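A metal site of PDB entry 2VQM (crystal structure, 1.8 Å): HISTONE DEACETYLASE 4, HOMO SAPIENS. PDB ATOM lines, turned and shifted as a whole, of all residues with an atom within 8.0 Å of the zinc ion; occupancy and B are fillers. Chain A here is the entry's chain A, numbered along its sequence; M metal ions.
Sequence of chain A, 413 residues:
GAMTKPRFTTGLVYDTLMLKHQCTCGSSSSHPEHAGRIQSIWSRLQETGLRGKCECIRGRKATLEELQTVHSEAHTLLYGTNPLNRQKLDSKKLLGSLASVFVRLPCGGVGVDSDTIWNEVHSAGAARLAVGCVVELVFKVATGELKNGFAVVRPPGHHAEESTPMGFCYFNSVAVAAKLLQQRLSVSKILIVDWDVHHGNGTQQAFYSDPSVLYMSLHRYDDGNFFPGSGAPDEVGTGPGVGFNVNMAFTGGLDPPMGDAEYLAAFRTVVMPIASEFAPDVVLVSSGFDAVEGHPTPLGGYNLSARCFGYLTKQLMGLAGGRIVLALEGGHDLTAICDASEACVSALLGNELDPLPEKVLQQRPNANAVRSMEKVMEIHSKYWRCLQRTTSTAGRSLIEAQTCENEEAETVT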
ATOM      1  N   HIS A  21      16.533  26.037  21.003  1.00  0.00           N
ATOM      2  CA  HIS A  21      16.032  25.003  20.089  1.00  0.00           C
ATOM      3  C   HIS A  21      17.164  24.329  19.304  1.00  0.00           C
ATOM      4  O   HIS A  21      17.849  24.971  18.510  1.00  0.00           O
ATOM      5  CB  HIS A  21      15.036  25.628  19.116  1.00  0.00           C
ATOM      6  CG  HIS A  21      14.639  24.707  18.012  1.00  0.00           C
ATOM      7  ND1 HIS A  21      13.906  23.553  18.227  1.00  0.00           N
ATOM      8  CD2 HIS A  21      14.862  24.767  16.671  1.00  0.00           C
ATOM      9  CE1 HIS A  21      13.711  22.939  17.070  1.00  0.00           C
ATOM     10  NE2 HIS A  21      14.272  23.659  16.117  1.00  0.00           N
ATOM     11  N   GLN A  22      17.326  23.033  19.534  1.00  0.00           N
ATOM     12  CA  GLN A  22      18.253  22.210  18.756  1.00  0.00           C
ATOM     13  C   GLN A  22      17.559  21.649  17.523  1.00  0.00           C
ATOM     14  O   GLN A  22      16.420  21.187  17.610  1.00  0.00           O
ATOM     15  CB  GLN A  22      18.794  21.068  19.606  1.00  0.00           C
ATOM     16  CG  GLN A  22      19.691  20.111  18.831  1.00  0.00           C
ATOM     17  CD  GLN A  22      20.643  19.387  19.727  1.00  0.00           C
ATOM     18  OE1 GLN A  22      20.312  19.044  20.865  1.00  0.00           O
ATOM     19  NE2 GLN A  22      21.857  19.143  19.232  1.00  0.00           N
ATOM     20  N   CYS A  23      18.261  21.686  16.397  1.00  0.00           N
ATOM     21  CA  CYS A  23      17.671  21.340  15.112  1.00  0.00           C
ATOM     22  C   CYS A  23      18.684  20.856  14.079  1.00  0.00           C
ATOM     23  O   CYS A  23      19.619  21.575  13.734  1.00  0.00           O
ATOM     24  CB  CYS A  23      16.959  22.556  14.536  1.00  0.00           C
ATOM     25  SG  CYS A  23      15.988  22.139  13.076  1.00  0.00           S
ATOM     26  N   THR A  24      18.469  19.645  13.568  1.00  0.00           N
ATOM     27  CA  THR A  24      19.319  19.078  12.516  1.00  0.00           C
ATOM     28  C   THR A  24      19.035  19.783  11.177  1.00  0.00           C
ATOM     29  O   THR A  24      17.882  20.086  10.860  1.00  0.00           O
ATOM     30  CB  THR A  24      19.073  17.569  12.381  1.00  0.00           C
ATOM     31  OG1 THR A  24      19.112  16.955  13.683  1.00  0.00           O
ATOM     32  CG2 THR A  24      20.123  16.927  11.475  1.00  0.00           C
ATOM     33  N   CYS A  25      20.105  20.036  10.412  1.00  0.00           N
ATOM     34  CA  CYS A  25      20.076  20.854   9.182  1.00  0.00           C
ATOM     35  C   CYS A  25      20.091  22.364   9.440  1.00  0.00           C
ATOM     36  O   CYS A  25      19.900  23.151   8.508  1.00  0.00           O
ATOM     37  CB  CYS A  25      18.889  20.534   8.252  1.00  0.00           C
ATOM     38  SG  CYS A  25      18.762  18.840   7.706  1.00  0.00           S
ATOM     39  N   GLY A  26      20.286  22.771  10.688  1.00  0.00           N
ATOM     40  CA  GLY A  26      20.378  24.190  11.030  1.00  0.00           C
ATOM     41  C   GLY A  26      21.706  24.780  10.600  1.00  0.00           C
ATOM     42  O   GLY A  26      21.781  25.568   9.654  1.00  0.00           O
ATOM     43  N   HIS A  34      16.656  30.343  11.044  1.00  0.00           N
ATOM     44  CA  HIS A  34      16.734  29.213  11.980  1.00  0.00           C
ATOM     45  C   HIS A  34      18.167  29.078  12.506  1.00  0.00           C
ATOM     46  O   HIS A  34      19.092  29.672  11.943  1.00  0.00           O
ATOM     47  CB  HIS A  34      16.303  27.915  11.263  1.00  0.00           C
ATOM     48  CG  HIS A  34      15.571  26.947  12.149  1.00  0.00           C
ATOM     49  ND1 HIS A  34      14.480  27.306  12.909  1.00  0.00           N
ATOM     50  CD2 HIS A  34      15.769  25.627  12.375  1.00  0.00           C
ATOM     51  CE1 HIS A  34      14.032  26.255  13.569  1.00  0.00           C
ATOM     52  NE2 HIS A  34      14.799  25.217  13.265  1.00  0.00           N
ATOM     53  N   ALA A  35      18.339  28.289  13.561  1.00  0.00           N
ATOM     54  CA  ALA A  35      19.661  28.003  14.149  1.00  0.00           C
ATOM     55  C   ALA A  35      20.375  29.268  14.641  1.00  0.00           C
ATOM     56  O   ALA A  35      20.749  30.137  13.845  1.00  0.00           O
ATOM     57  CB  ALA A  35      20.542  27.229  13.164  1.00  0.00           C
ATOM     58  N   GLN A  39      25.029  27.203  18.043  1.00  0.00           N
ATOM     59  CA  GLN A  39      24.734  26.041  17.197  1.00  0.00           C
ATOM     60  C   GLN A  39      25.381  26.199  15.823  1.00  0.00           C
ATOM     61  O   GLN A  39      25.936  25.251  15.277  1.00  0.00           O
ATOM     62  CB  GLN A  39      23.215  25.806  17.091  1.00  0.00           C
ATOM     63  CG  GLN A  39      22.834  24.438  16.520  1.00  0.00           C
ATOM     64  CD  GLN A  39      21.343  24.122  16.646  1.00  0.00           C
ATOM     65  OE1 GLN A  39      20.486  25.027  16.692  1.00  0.00           O
ATOM     66  NE2 GLN A  39      21.034  22.843  16.735  1.00  0.00           N
ATOM     67  N   LEU A 105       7.649  24.121  16.148  1.00  0.00           N
ATOM     68  CA  LEU A 105       8.231  25.018  15.145  1.00  0.00           C
ATOM     69  C   LEU A 105       8.000  24.520  13.715  1.00  0.00           C
ATOM     70  O   LEU A 105       7.714  23.334  13.508  1.00  0.00           O
ATOM     71  CB  LEU A 105       9.745  25.166  15.408  1.00  0.00           C
ATOM     72  CG  LEU A 105      10.150  25.958  16.649  1.00  0.00           C
ATOM     73  CD1 LEU A 105      11.668  25.942  16.811  1.00  0.00           C
ATOM     74  CD2 LEU A 105       9.642  27.394  16.597  1.00  0.00           C
ATOM     75  N   PRO A 106       8.110  25.422  12.703  1.00  0.00           N
ATOM     76  CA  PRO A 106       7.903  25.055  11.292  1.00  0.00           C
ATOM     77  C   PRO A 106       8.831  23.965  10.719  1.00  0.00           C
ATOM     78  O   PRO A 106       8.590  23.477   9.606  1.00  0.00           O
ATOM     79  CB  PRO A 106       8.099  26.385  10.542  1.00  0.00           C
ATOM     80  CG  PRO A 106       8.806  27.276  11.475  1.00  0.00           C
ATOM     81  CD  PRO A 106       8.405  26.861  12.849  1.00  0.00           C
ATOM     82  N   CYS A 107       9.873  23.595  11.449  1.00  0.00           N
ATOM     83  CA  CYS A 107      10.724  22.468  11.071  1.00  0.00           C
ATOM     84  C   CYS A 107      10.158  21.134  11.580  1.00  0.00           C
ATOM     85  O   CYS A 107      10.665  20.069  11.216  1.00  0.00           O
ATOM     86  CB  CYS A 107      12.129  22.673  11.638  1.00  0.00           C
ATOM     87  SG  CYS A 107      12.152  22.882  13.445  1.00  0.00           S
ATOM     88  N   GLY A 108       9.127  21.190  12.409  1.00  0.00           N
ATOM     89  CA  GLY A 108       8.577  19.991  13.061  1.00  0.00           C
ATOM     90  C   GLY A 108       9.233  19.691  14.409  1.00  0.00           C
ATOM     91  O   GLY A 108       8.895  18.691  15.050  1.00  0.00           O
ATOM     92  N   GLY A 109      10.158  20.549  14.816  1.00  0.00           N
ATOM     93  CA  GLY A 109      10.813  20.421  16.120  1.00  0.00           C
ATOM     94  C   GLY A 109      10.143  21.289  17.172  1.00  0.00           C
ATOM     95  O   GLY A 109       9.245  22.078  16.864  1.00  0.00           O
ATOM     96  N   VAL A 110      10.586  21.152  18.412  1.00  0.00           N
ATOM     97  CA  VAL A 110      10.072  21.948  19.518  1.00  0.00           C
ATOM     98  C   VAL A 110      11.197  22.813  20.106  1.00  0.00           C
ATOM     99  O   VAL A 110      12.367  22.441  20.061  1.00  0.00           O
ATOM    100  CB  VAL A 110       9.459  21.059  20.628  1.00  0.00           C
ATOM    101  CG1 VAL A 110      10.556  20.384  21.451  1.00  0.00           C
ATOM    102  CG2 VAL A 110       8.541  21.886  21.518  1.00  0.00           C
ATOM    103  N   GLY A 111      10.811  23.969  20.650  1.00  0.00           N
ATOM    104  CA  GLY A 111      11.760  24.834  21.338  1.00  0.00           C
ATOM    105  C   GLY A 111      11.135  25.596  22.495  1.00  0.00           C
ATOM    106  O   GLY A 111       9.908  25.595  22.666  1.00  0.00           O
HETATM  107 ZN    ZN M   1      14.234  23.546  13.962  1.00  0.00          ZN
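A ring nitrogen (ND1) of His 21 lies within hydrogen-bond range of the backbone carbonyl oxygen (O) of Val 110 (2.6 Å).
The side-chain amide oxygen (OE1) of Gln 39 sits close to the backbone carbonyl oxygen (O) of His 21 (3.2 Å).
The backbone NH (N) of Gly 109 sits close to the side-chain sulfur (SG) of Cys 107 (3.4 Å).
The side-chain amide nitrogen of Gln 39 lies close to the backbone NH of Cys 23.
The zinc ion is bound by NE2 of His 34 (1.9 Å), NE2 of His 21 (2.2 Å), SG of Cys 107 (2.2 Å) and SG of Cys 23 (2.4 Å).
The zinc ion has four donor atoms within binding distance.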
